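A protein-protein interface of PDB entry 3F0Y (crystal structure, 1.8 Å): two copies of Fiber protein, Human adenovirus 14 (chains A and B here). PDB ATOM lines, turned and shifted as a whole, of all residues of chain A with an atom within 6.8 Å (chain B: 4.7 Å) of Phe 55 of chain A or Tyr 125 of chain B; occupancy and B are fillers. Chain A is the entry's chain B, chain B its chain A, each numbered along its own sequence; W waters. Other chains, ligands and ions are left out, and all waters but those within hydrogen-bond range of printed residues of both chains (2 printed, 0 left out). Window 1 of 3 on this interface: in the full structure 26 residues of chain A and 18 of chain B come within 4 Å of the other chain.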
ATOM      1  N   VAL A  21      19.828  20.489  -2.117  1.00  0.00           N
ATOM      2  CA  VAL A  21      20.818  21.435  -2.613  1.00  0.00           C
ATOM      3  C   VAL A  21      22.220  20.964  -2.255  1.00  0.00           C
ATOM      4  O   VAL A  21      22.474  20.564  -1.119  1.00  0.00           O
ATOM      5  CB  VAL A  21      20.595  22.837  -2.018  1.00  0.00           C
ATOM      6  CG1 VAL A  21      21.697  23.788  -2.467  1.00  0.00           C
ATOM      7  CG2 VAL A  21      19.227  23.366  -2.417  1.00  0.00           C
ATOM      8  N   ILE A  42      21.873  17.900  -9.646  1.00  0.00           N
ATOM      9  CA  ILE A  42      20.904  18.712  -8.933  1.00  0.00           C
ATOM     10  C   ILE A  42      19.660  18.765  -9.805  1.00  0.00           C
ATOM     11  O   ILE A  42      19.694  19.310 -10.907  1.00  0.00           O
ATOM     12  CB  ILE A  42      21.435  20.133  -8.650  1.00  0.00           C
ATOM     13  CG1 ILE A  42      22.838  20.077  -8.026  1.00  0.00           C
ATOM     14  CG2 ILE A  42      20.481  20.889  -7.736  1.00  0.00           C
ATOM     15  CD1 ILE A  42      22.925  19.278  -6.738  1.00  0.00           C
ATOM     16  N   LEU A  43      18.580  18.158  -9.320  1.00  0.00           N
ATOM     17  CA  LEU A  43      17.328  18.074 -10.063  1.00  0.00           C
ATOM     18  C   LEU A  43      16.186  18.480  -9.145  1.00  0.00           C
ATOM     19  O   LEU A  43      16.042  17.931  -8.054  1.00  0.00           O
ATOM     20  CB  LEU A  43      17.106  16.647 -10.576  1.00  0.00           C
ATOM     21  CG  LEU A  43      15.788  16.370 -11.309  1.00  0.00           C
ATOM     22  CD1 LEU A  43      15.722  17.151 -12.613  1.00  0.00           C
ATOM     23  CD2 LEU A  43      15.621  14.880 -11.565  1.00  0.00           C
ATOM     24  N   THR A  44      15.393  19.448  -9.588  1.00  0.00           N
ATOM     25  CA  THR A  44      14.218  19.892  -8.855  1.00  0.00           C
ATOM     26  C   THR A  44      12.998  19.811  -9.770  1.00  0.00           C
ATOM     27  O   THR A  44      12.975  20.414 -10.841  1.00  0.00           O
ATOM     28  CB  THR A  44      14.408  21.329  -8.337  1.00  0.00           C
ATOM     29  OG1 THR A  44      15.596  21.391  -7.537  1.00  0.00           O
ATOM     30  CG2 THR A  44      13.210  21.781  -7.508  1.00  0.00           C
ATOM     31  N   LEU A  45      12.001  19.039  -9.349  1.00  0.00           N
ATOM     32  CA  LEU A  45      10.742  18.918 -10.074  1.00  0.00           C
ATOM     33  C   LEU A  45       9.667  19.595  -9.240  1.00  0.00           C
ATOM     34  O   LEU A  45       9.456  19.220  -8.090  1.00  0.00           O
ATOM     35  CB  LEU A  45      10.376  17.448 -10.286  1.00  0.00           C
ATOM     36  CG  LEU A  45      11.412  16.570 -10.989  1.00  0.00           C
ATOM     37  CD1 LEU A  45      10.944  15.121 -11.011  1.00  0.00           C
ATOM     38  CD2 LEU A  45      11.682  17.072 -12.399  1.00  0.00           C
ATOM     39  N   VAL A  46       9.015  20.603  -9.814  1.00  0.00           N
ATOM     40  CA  VAL A  46       7.972  21.352  -9.122  1.00  0.00           C
ATOM     41  C   VAL A  46       6.653  21.231  -9.875  1.00  0.00           C
ATOM     42  O   VAL A  46       6.587  21.502 -11.072  1.00  0.00           O
ATOM     43  CB  VAL A  46       8.342  22.846  -8.984  1.00  0.00           C
ATOM     44  CG1 VAL A  46       7.231  23.609  -8.272  1.00  0.00           C
ATOM     45  CG2 VAL A  46       9.659  23.001  -8.236  1.00  0.00           C
ATOM     46  N   VAL A  52       4.981  20.014 -14.912  1.00  0.00           N
ATOM     47  CA  VAL A  52       6.098  19.988 -13.985  1.00  0.00           C
ATOM     48  C   VAL A  52       7.120  20.990 -14.498  1.00  0.00           C
ATOM     49  O   VAL A  52       7.420  21.015 -15.691  1.00  0.00           O
ATOM     50  CB  VAL A  52       6.741  18.586 -13.901  1.00  0.00           C
ATOM     51  CG1 VAL A  52       8.144  18.659 -13.289  1.00  0.00           C
ATOM     52  CG2 VAL A  52       5.855  17.647 -13.098  1.00  0.00           C
ATOM     53  N   THR A  53       7.620  21.835 -13.603  1.00  0.00           N
ATOM     54  CA  THR A  53       8.766  22.682 -13.894  1.00  0.00           C
ATOM     55  C   THR A  53       9.994  21.902 -13.449  1.00  0.00           C
ATOM     56  O   THR A  53      10.167  21.646 -12.257  1.00  0.00           O
ATOM     57  CB  THR A  53       8.688  24.025 -13.144  1.00  0.00           C
ATOM     58  OG1 THR A  53       7.475  24.699 -13.496  1.00  0.00           O
ATOM     59  CG2 THR A  53       9.868  24.911 -13.501  1.00  0.00           C
ATOM     60  N   ALA A  54      10.817  21.497 -14.413  1.00  0.00           N
ATOM     61  CA  ALA A  54      11.987  20.667 -14.145  1.00  0.00           C
ATOM     62  C   ALA A  54      13.239  21.527 -14.215  1.00  0.00           C
ATOM     63  O   ALA A  54      13.463  22.209 -15.207  1.00  0.00           O
ATOM     64  CB  ALA A  54      12.064  19.532 -15.144  1.00  0.00           C
ATOM     65  N   PHE A  55      14.048  21.475 -13.159  1.00  0.00           N
ATOM     66  CA  PHE A  55      15.179  22.381 -12.963  1.00  0.00           C
ATOM     67  C   PHE A  55      16.407  21.522 -12.682  1.00  0.00           C
ATOM     68  O   PHE A  55      16.480  20.868 -11.643  1.00  0.00           O
ATOM     69  CB  PHE A  55      14.849  23.299 -11.784  1.00  0.00           C
ATOM     70  CG  PHE A  55      15.941  24.257 -11.397  1.00  0.00           C
ATOM     71  CD1 PHE A  55      16.049  25.495 -12.011  1.00  0.00           C
ATOM     72  CD2 PHE A  55      16.816  23.947 -10.363  1.00  0.00           C
ATOM     73  CE1 PHE A  55      17.036  26.398 -11.626  1.00  0.00           C
ATOM     74  CE2 PHE A  55      17.805  24.841  -9.976  1.00  0.00           C
ATOM     75  CZ  PHE A  55      17.914  26.067 -10.606  1.00  0.00           C
ATOM     76  N   VAL A  56      17.360  21.511 -13.612  1.00  0.00           N
ATOM     77  CA  VAL A  56      18.447  20.535 -13.561  1.00  0.00           C
ATOM     78  C   VAL A  56      19.814  21.121 -13.907  1.00  0.00           C
ATOM     79  O   VAL A  56      19.949  21.936 -14.819  1.00  0.00           O
ATOM     80  CB  VAL A  56      18.159  19.338 -14.501  1.00  0.00           C
ATOM     81  CG1 VAL A  56      18.155  19.785 -15.962  1.00  0.00           C
ATOM     82  CG2 VAL A  56      19.171  18.216 -14.277  1.00  0.00           C
ATOM     83  N   TYR A  57      20.825  20.699 -13.159  1.00  0.00           N
ATOM     84  CA  TYR A  57      22.209  20.953 -13.540  1.00  0.00           C
ATOM     85  C   TYR A  57      23.152  19.946 -12.902  1.00  0.00           C
ATOM     86  O   TYR A  57      22.742  19.127 -12.074  1.00  0.00           O
ATOM     87  CB  TYR A  57      22.625  22.393 -13.223  1.00  0.00           C
ATOM     88  CG  TYR A  57      22.533  22.805 -11.771  1.00  0.00           C
ATOM     89  CD1 TYR A  57      21.310  23.144 -11.198  1.00  0.00           C
ATOM     90  CD2 TYR A  57      23.675  22.895 -10.981  1.00  0.00           C
ATOM     91  CE1 TYR A  57      21.229  23.536  -9.869  1.00  0.00           C
ATOM     92  CE2 TYR A  57      23.604  23.287  -9.660  1.00  0.00           C
ATOM     93  CZ  TYR A  57      22.379  23.608  -9.107  1.00  0.00           C
ATOM     94  OH  TYR A  57      22.305  24.002  -7.790  1.00  0.00           O
ATOM     95  N   GLN A 105      16.867  23.178   2.673  1.00  0.00           N
ATOM     96  CA  GLN A 105      17.769  23.021   1.530  1.00  0.00           C
ATOM     97  C   GLN A 105      18.065  21.550   1.227  1.00  0.00           C
ATOM     98  O   GLN A 105      18.833  21.245   0.315  1.00  0.00           O
ATOM     99  CB  GLN A 105      19.083  23.766   1.792  1.00  0.00           C
ATOM    100  CG  GLN A 105      18.911  25.251   2.069  1.00  0.00           C
ATOM    101  CD  GLN A 105      18.333  26.001   0.884  1.00  0.00           C
ATOM    102  OE1 GLN A 105      17.273  26.620   0.982  1.00  0.00           O
ATOM    103  NE2 GLN A 105      19.019  25.938  -0.246  1.00  0.00           N
ATOM    104  N   PRO A 198      21.956  26.117 -14.583  1.00  0.00           N
ATOM    105  CA  PRO A 198      20.648  25.475 -14.487  1.00  0.00           C
ATOM    106  C   PRO A 198      19.843  25.531 -15.782  1.00  0.00           C
ATOM    107  O   PRO A 198      19.751  26.587 -16.415  1.00  0.00           O
ATOM    108  CB  PRO A 198      19.944  26.268 -13.384  1.00  0.00           C
ATOM    109  CG  PRO A 198      21.021  26.896 -12.607  1.00  0.00           C
ATOM    110  CD  PRO A 198      22.119  27.177 -13.572  1.00  0.00           C
ATOM    111  N   PHE A 199      19.292  24.385 -16.169  1.00  0.00           N
ATOM    112  CA  PHE A 199      18.383  24.300 -17.295  1.00  0.00           C
ATOM    113  C   PHE A 199      16.993  23.990 -16.771  1.00  0.00           C
ATOM    114  O   PHE A 199      16.809  23.058 -15.987  1.00  0.00           O
ATOM    115  CB  PHE A 199      18.814  23.212 -18.272  1.00  0.00           C
ATOM    116  CG  PHE A 199      17.830  22.980 -19.386  1.00  0.00           C
ATOM    117  CD1 PHE A 199      17.492  24.012 -20.250  1.00  0.00           C
ATOM    118  CD2 PHE A 199      17.240  21.735 -19.568  1.00  0.00           C
ATOM    119  CE1 PHE A 199      16.584  23.810 -21.275  1.00  0.00           C
ATOM    120  CE2 PHE A 199      16.334  21.527 -20.597  1.00  0.00           C
ATOM    121  CZ  PHE A 199      16.008  22.567 -21.451  1.00  0.00           C
ATOM    122  N   THR A 200      16.023  24.785 -17.209  1.00  0.00           N
ATOM    123  CA  THR A 200      14.640  24.599 -16.818  1.00  0.00           C
ATOM    124  C   THR A 200      13.828  24.168 -18.029  1.00  0.00           C
ATOM    125  O   THR A 200      13.860  24.827 -19.068  1.00  0.00           O
ATOM    126  CB  THR A 200      14.048  25.889 -16.239  1.00  0.00           C
ATOM    127  OG1 THR A 200      14.797  26.274 -15.083  1.00  0.00           O
ATOM    128  CG2 THR A 200      12.588  25.688 -15.844  1.00  0.00           C
ATOM    129  N   PHE A 201      13.120  23.050 -17.893  1.00  0.00           N
ATOM    130  CA  PHE A 201      12.188  22.603 -18.919  1.00  0.00           C
ATOM    131  C   PHE A 201      10.845  22.244 -18.304  1.00  0.00           C
ATOM    132  O   PHE A 201      10.695  22.202 -17.079  1.00  0.00           O
ATOM    133  CB  PHE A 201      12.759  21.436 -19.739  1.00  0.00           C
ATOM    134  CG  PHE A 201      13.047  20.192 -18.941  1.00  0.00           C
ATOM    135  CD1 PHE A 201      12.186  19.104 -18.994  1.00  0.00           C
ATOM    136  CD2 PHE A 201      14.201  20.092 -18.173  1.00  0.00           C
ATOM    137  CE1 PHE A 201      12.456  17.944 -18.278  1.00  0.00           C
ATOM    138  CE2 PHE A 201      14.479  18.935 -17.453  1.00  0.00           C
ATOM    139  CZ  PHE A 201      13.605  17.860 -17.505  1.00  0.00           C
ATOM    140  N   LEU B  51      11.751  26.632  -5.833  1.00  0.00           N
ATOM    141  CA  LEU B  51      12.370  27.621  -6.707  1.00  0.00           C
ATOM    142  C   LEU B  51      11.661  28.964  -6.653  1.00  0.00           C
ATOM    143  O   LEU B  51      10.521  29.065  -6.200  1.00  0.00           O
ATOM    144  CB  LEU B  51      12.342  27.128  -8.155  1.00  0.00           C
ATOM    145  CG  LEU B  51      12.918  25.741  -8.434  1.00  0.00           C
ATOM    146  CD1 LEU B  51      12.794  25.424  -9.912  1.00  0.00           C
ATOM    147  CD2 LEU B  51      14.364  25.662  -7.983  1.00  0.00           C
ATOM    148  N   PRO B 120      17.798  34.359  -3.241  1.00  0.00           N
ATOM    149  CA  PRO B 120      18.617  33.246  -3.717  1.00  0.00           C
ATOM    150  C   PRO B 120      19.320  32.551  -2.557  1.00  0.00           C
ATOM    151  O   PRO B 120      19.949  33.211  -1.727  1.00  0.00           O
ATOM    152  CB  PRO B 120      19.633  33.924  -4.644  1.00  0.00           C
ATOM    153  CG  PRO B 120      19.706  35.323  -4.172  1.00  0.00           C
ATOM    154  CD  PRO B 120      18.333  35.661  -3.679  1.00  0.00           C
ATOM    155  N   SER B 121      19.186  31.228  -2.499  1.00  0.00           N
ATOM    156  CA  SER B 121      19.768  30.429  -1.428  1.00  0.00           C
ATOM    157  C   SER B 121      21.274  30.640  -1.318  1.00  0.00           C
ATOM    158  O   SER B 121      21.995  30.534  -2.308  1.00  0.00           O
ATOM    159  CB  SER B 121      19.479  28.942  -1.662  1.00  0.00           C
ATOM    160  OG  SER B 121      20.279  28.129  -0.823  1.00  0.00           O
ATOM    161  N   THR B 122      21.744  30.936  -0.109  1.00  0.00           N
ATOM    162  CA  THR B 122      23.181  31.019   0.155  1.00  0.00           C
ATOM    163  C   THR B 122      23.811  29.626   0.191  1.00  0.00           C
ATOM    164  O   THR B 122      25.028  29.491   0.090  1.00  0.00           O
ATOM    165  CB  THR B 122      23.483  31.759   1.472  1.00  0.00           C
ATOM    166  OG1 THR B 122      22.774  31.139   2.550  1.00  0.00           O
ATOM    167  CG2 THR B 122      23.071  33.222   1.368  1.00  0.00           C
ATOM    168  N   THR B 123      22.981  28.594   0.338  1.00  0.00           N
ATOM    169  CA  THR B 123      23.444  27.214   0.248  1.00  0.00           C
ATOM    170  C   THR B 123      23.667  26.820  -1.209  1.00  0.00           C
ATOM    171  O   THR B 123      24.656  26.174  -1.524  1.00  0.00           O
ATOM    172  CB  THR B 123      22.454  26.233   0.906  1.00  0.00           C
ATOM    173  OG1 THR B 123      22.203  26.646   2.255  1.00  0.00           O
ATOM    174  CG2 THR B 123      23.019  24.820   0.911  1.00  0.00           C
ATOM    175  N   ALA B 124      22.748  27.213  -2.088  1.00  0.00           N
ATOM    176  CA  ALA B 124      22.879  26.945  -3.522  1.00  0.00           C
ATOM    177  C   ALA B 124      23.854  27.916  -4.187  1.00  0.00           C
ATOM    178  O   ALA B 124      24.604  27.530  -5.086  1.00  0.00           O
ATOM    179  CB  ALA B 124      21.516  27.026  -4.203  1.00  0.00           C
ATOM    180  N   TYR B 125      23.831  29.169  -3.735  1.00  0.00           N
ATOM    181  CA  TYR B 125      24.628  30.250  -4.319  1.00  0.00           C
ATOM    182  C   TYR B 125      25.436  30.929  -3.210  1.00  0.00           C
ATOM    183  O   TYR B 125      24.995  31.923  -2.623  1.00  0.00           O
ATOM    184  CB  TYR B 125      23.705  31.240  -5.039  1.00  0.00           C
ATOM    185  CG  TYR B 125      22.645  30.528  -5.846  1.00  0.00           C
ATOM    186  CD1 TYR B 125      21.319  30.505  -5.428  1.00  0.00           C
ATOM    187  CD2 TYR B 125      22.982  29.830  -6.999  1.00  0.00           C
ATOM    188  CE1 TYR B 125      20.353  29.830  -6.151  1.00  0.00           C
ATOM    189  CE2 TYR B 125      22.022  29.153  -7.731  1.00  0.00           C
ATOM    190  CZ  TYR B 125      20.708  29.155  -7.300  1.00  0.00           C
ATOM    191  OH  TYR B 125      19.744  28.485  -8.014  1.00  0.00           O
ATOM    192  N   PRO B 126      26.621  30.377  -2.905  1.00  0.00           N
ATOM    193  CA  PRO B 126      27.395  30.851  -1.765  1.00  0.00           C
ATOM    194  C   PRO B 126      28.065  32.201  -1.988  1.00  0.00           C
ATOM    195  O   PRO B 126      28.124  32.691  -3.118  1.00  0.00           O
ATOM    196  CB  PRO B 126      28.452  29.758  -1.584  1.00  0.00           C
ATOM    197  CG  PRO B 126      28.622  29.171  -2.926  1.00  0.00           C
ATOM    198  CD  PRO B 126      27.295  29.270  -3.608  1.00  0.00           C
ATOM    199  N   PHE B 127      28.539  32.791  -0.895  1.00  0.00           N
ATOM    200  CA  PHE B 127      29.385  33.977  -0.944  1.00  0.00           C
ATOM    201  C   PHE B 127      30.829  33.563  -0.705  1.00  0.00           C
ATOM    202  O   PHE B 127      31.098  32.687   0.121  1.00  0.00           O
ATOM    203  CB  PHE B 127      28.978  34.989   0.129  1.00  0.00           C
ATOM    204  CG  PHE B 127      27.765  35.793  -0.221  1.00  0.00           C
ATOM    205  CD1 PHE B 127      26.504  35.377   0.178  1.00  0.00           C
ATOM    206  CD2 PHE B 127      27.884  36.973  -0.940  1.00  0.00           C
ATOM    207  CE1 PHE B 127      25.384  36.120  -0.135  1.00  0.00           C
ATOM    208  CE2 PHE B 127      26.765  37.723  -1.262  1.00  0.00           C
ATOM    209  CZ  PHE B 127      25.511  37.296  -0.859  1.00  0.00           C
ATOM    210  N   GLU B 135      28.720  28.067  -9.775  1.00  0.00           N
ATOM    211  CA  GLU B 135      27.319  27.769  -9.466  1.00  0.00           C
ATOM    212  C   GLU B 135      26.469  29.029  -9.276  1.00  0.00           C
ATOM    213  O   GLU B 135      25.241  28.963  -9.319  1.00  0.00           O
ATOM    214  CB  GLU B 135      27.235  26.882  -8.220  1.00  0.00           C
ATOM    215  CG  GLU B 135      27.903  25.523  -8.401  1.00  0.00           C
ATOM    216  CD  GLU B 135      27.981  24.730  -7.114  1.00  0.00           C
ATOM    217  OE1 GLU B 135      26.946  24.601  -6.433  1.00  0.00           O
ATOM    218  OE2 GLU B 135      29.074  24.222  -6.791  1.00  0.00           O
ATOM    219  N   ASN B 136      27.127  30.170  -9.081  1.00  0.00           N
ATOM    220  CA  ASN B 136      26.443  31.447  -8.887  1.00  0.00           C
ATOM    221  C   ASN B 136      25.909  32.078 -10.176  1.00  0.00           C
ATOM    222  O   ASN B 136      25.195  33.078 -10.117  1.00  0.00           O
ATOM    223  CB  ASN B 136      27.383  32.439  -8.194  1.00  0.00           C
ATOM    224  CG  ASN B 136      27.754  32.004  -6.792  1.00  0.00           C
ATOM    225  OD1 ASN B 136      28.788  31.375  -6.577  1.00  0.00           O
ATOM    226  ND2 ASN B 136      26.901  32.325  -5.828  1.00  0.00           N
ATOM    227  N   LEU B 160      24.092  35.273  -8.806  1.00  0.00           N
ATOM    228  CA  LEU B 160      23.416  35.265  -7.517  1.00  0.00           C
ATOM    229  C   LEU B 160      24.452  35.244  -6.406  1.00  0.00           C
ATOM    230  O   LEU B 160      25.382  34.440  -6.438  1.00  0.00           O
ATOM    231  CB  LEU B 160      22.505  34.044  -7.408  1.00  0.00           C
ATOM    232  CG  LEU B 160      21.461  33.915  -8.518  1.00  0.00           C
ATOM    233  CD1 LEU B 160      20.661  32.637  -8.348  1.00  0.00           C
ATOM    234  CD2 LEU B 160      20.544  35.125  -8.543  1.00  0.00           C
ATOM    235  N   ASN B 161      24.284  36.132  -5.428  1.00  0.00           N
ATOM    236  CA  ASN B 161      25.170  36.212  -4.269  1.00  0.00           C
ATOM    237  C   ASN B 161      26.645  36.367  -4.676  1.00  0.00           C
ATOM    238  O   ASN B 161      27.004  37.389  -5.256  1.00  0.00           O
ATOM    239  CB  ASN B 161      24.924  35.014  -3.343  1.00  0.00           C
ATOM    240  CG  ASN B 161      23.512  35.000  -2.775  1.00  0.00           C
ATOM    241  OD1 ASN B 161      22.850  36.035  -2.704  1.00  0.00           O
ATOM    242  ND2 ASN B 161      23.046  33.824  -2.371  1.00  0.00           N
ATOM    243  N   GLN B 162      27.480  35.367  -4.383  1.00  0.00           N
ATOM    244  CA  GLN B 162      28.909  35.361  -4.741  1.00  0.00           C
ATOM    245  C   GLN B 162      29.753  36.369  -3.959  1.00  0.00           C
ATOM    246  O   GLN B 162      30.690  35.983  -3.259  1.00  0.00           O
ATOM    247  CB  GLN B 162      29.116  35.548  -6.256  1.00  0.00           C
ATOM    248  CG  GLN B 162      30.579  35.565  -6.700  1.00  0.00           C
ATOM    249  CD  GLN B 162      31.379  34.403  -6.147  1.00  0.00           C
ATOM    250  OE1 GLN B 162      30.979  33.248  -6.275  1.00  0.00           O
ATOM    251  NE2 GLN B 162      32.515  34.705  -5.527  1.00  0.00           N
ATOM    252  N   TYR B 202      15.337  30.910 -13.152  1.00  0.00           N
ATOM    253  CA  TYR B 202      14.946  30.193 -11.948  1.00  0.00           C
ATOM    254  C   TYR B 202      16.137  30.022 -11.017  1.00  0.00           C
ATOM    255  O   TYR B 202      17.275  29.883 -11.464  1.00  0.00           O
ATOM    256  CB  TYR B 202      14.355  28.831 -12.319  1.00  0.00           C
ATOM    257  CG  TYR B 202      13.388  28.905 -13.477  1.00  0.00           C
ATOM    258  CD1 TYR B 202      12.013  28.907 -13.268  1.00  0.00           C
ATOM    259  CD2 TYR B 202      13.853  29.003 -14.787  1.00  0.00           C
ATOM    260  CE1 TYR B 202      11.130  28.988 -14.335  1.00  0.00           C
ATOM    261  CE2 TYR B 202      12.984  29.084 -15.854  1.00  0.00           C
ATOM    262  CZ  TYR B 202      11.625  29.077 -15.624  1.00  0.00           C
ATOM    263  OH  TYR B 202      10.767  29.158 -16.692  1.00  0.00           O
ATOM    264  N   TYR B 203      15.865  30.048  -9.719  1.00  0.00           N
ATOM    265  CA  TYR B 203      16.896  29.791  -8.737  1.00  0.00           C
ATOM    266  C   TYR B 203      16.308  29.168  -7.483  1.00  0.00           C
ATOM    267  O   TYR B 203      15.130  29.364  -7.171  1.00  0.00           O
ATOM    268  CB  TYR B 203      17.705  31.055  -8.419  1.00  0.00           C
ATOM    269  CG  TYR B 203      16.936  32.227  -7.841  1.00  0.00           C
ATOM    270  CD1 TYR B 203      16.584  32.260  -6.495  1.00  0.00           C
ATOM    271  CD2 TYR B 203      16.606  33.325  -8.631  1.00  0.00           C
ATOM    272  CE1 TYR B 203      15.901  33.345  -5.955  1.00  0.00           C
ATOM    273  CE2 TYR B 203      15.923  34.416  -8.101  1.00  0.00           C
ATOM    274  CZ  TYR B 203      15.574  34.418  -6.762  1.00  0.00           C
ATOM    275  OH  TYR B 203      14.902  35.494  -6.229  1.00  0.00           O
ATOM    276  N   ILE B 204      17.140  28.401  -6.786  1.00  0.00           N
ATOM    277  CA  ILE B 204      16.741  27.733  -5.558  1.00  0.00           C
ATOM    278  C   ILE B 204      16.629  28.790  -4.475  1.00  0.00           C
ATOM    279  O   ILE B 204      17.572  29.545  -4.232  1.00  0.00           O
ATOM    280  CB  ILE B 204      17.757  26.656  -5.143  1.00  0.00           C
ATOM    281  CG1 ILE B 204      17.810  25.545  -6.196  1.00  0.00           C
ATOM    282  CG2 ILE B 204      17.394  26.076  -3.781  1.00  0.00           C
ATOM    283  CD1 ILE B 204      18.967  24.592  -6.022  1.00  0.00           C
HETATM  284  O   HOH W   1      21.007  26.555  -9.271  1.00  0.00           O
HETATM  285  O   HOH W   2      24.383  25.374  -6.762  1.00  0.00           O
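The side-chain hydroxyl (OG) of Ser 121 of chain B is in hydrogen-bond range of the side-chain amide nitrogen (NE2) of Gln 105 of chain A (2.6 Å).
The backbone carbonyl oxygen (O) of Ser 121 of chain B sits at hydrogen-bond distance from the side-chain amide nitrogen (ND2) of Asn 161 of chain B (3.5 Å). O of Ile 204 of chain B is in hydrogen-bond range of N of Ser 121 of chain B (2.9 Å). ND2 of Asn 161 of chain B is in hydrogen-bond range of O of Tyr 125 of chain B (2.7 Å). The side-chain hydroxyl (OH) of Tyr 125 of chain B is in hydrogen-bond range of the backbone NH (N) of Ile 204 of chain B, 2.9 Å away. N of Ile 42 of chain A is in hydrogen-bond range of O of Tyr 57 of chain A (2.9 Å). O of Phe 55 of chain A is in hydrogen-bond range of N of Thr 44 of chain A (2.7 Å).
Among the printed residues, pairs that only touch across the chains: Thr 200 of chain A with Tyr 202 of chain B (2.9 Å), Phe 55 of chain A with Tyr 202 of chain B (3.5 Å), Phe 55 of chain A with Leu 51 of chain B (3.5 Å), Val 21 of chain A with Ala 124 of chain B (3.5 Å), Val 21 of chain A with Ile 204 of chain B (3.5 Å), Gln 105 of chain A with Thr 123 of chain B (3.6 Å), Val 21 of chain A with Thr 123 of chain B (3.8 Å), Tyr 57 of chain A with Ile 204 of chain B (3.8 Å), Phe 55 of chain A with Ile 204 of chain B (3.8 Å), Gln 105 of chain A with Ile 204 of chain B (3.9 Å) and Phe 55 of chain A with Tyr 125 of chain B (3.99 Å).
Of the printed residues of chain B, Val 21 of chain A touches Thr 123, Ala 124 and Ile 204. Of the printed residues of chain B, Phe 55 of chain A touches Leu 51, Tyr 125, Tyr 202 and Ile 204. Printed residues of chain B within 4 Å of Gln 105 of chain A: Ser 121 (2.6 Å), Thr 123 (3.6 Å) and Ile 204 (3.9 Å). Pro 198 of chain A touches none of the printed residues of chain B. Printed residues of chain A within 4 Å of Ser 121 of chain B: Gln 105 (2.6 Å). Of the printed residues of chain A, Tyr 125 of chain B touches Phe 55 (3.99 Å). The nearest printed residue of chain B that does not touch Phe 55 of chain A is Tyr 203 of chain B (4.3 Å). The nearest printed residue of chain A that does not touch Tyr 125 of chain B is Pro 198 of chain A (5.0 Å). The nearest printed residue of chain B that does not touch Thr 200 of chain A is Leu 51 of chain B (5.6 Å).
Of the 17 printed residues of chain B, 7 touch a printed residue of chain A. Of the 17 printed residues of chain A, 5 touch a printed residue of chain B. Hydrophobic or aromatic side chains of chain A within 4 Å of the printed part of chain B: Val 21, Phe 55 and Tyr 57. Among the printed residues, no Asp or Glu carboxylate lies within 4 Å of a Lys or Arg side-chain nitrogen of the other chain.
No position is printed for both chains. Of the 12 pairs that touch across the chains among the printed residues, none has its exchanged pair printed and touching as well.
Water W1 bridges OH of Tyr 125 of chain B (2.6 Å) and OH of Tyr 57 of chain A (3.2 Å). Water W2 lies within hydrogen-bond range of OH of Tyr 57 of chain A (2.7 Å), OE1 of Glu 135 of chain B (2.7 Å) and O of Ala 124 of chain B (2.7 Å).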
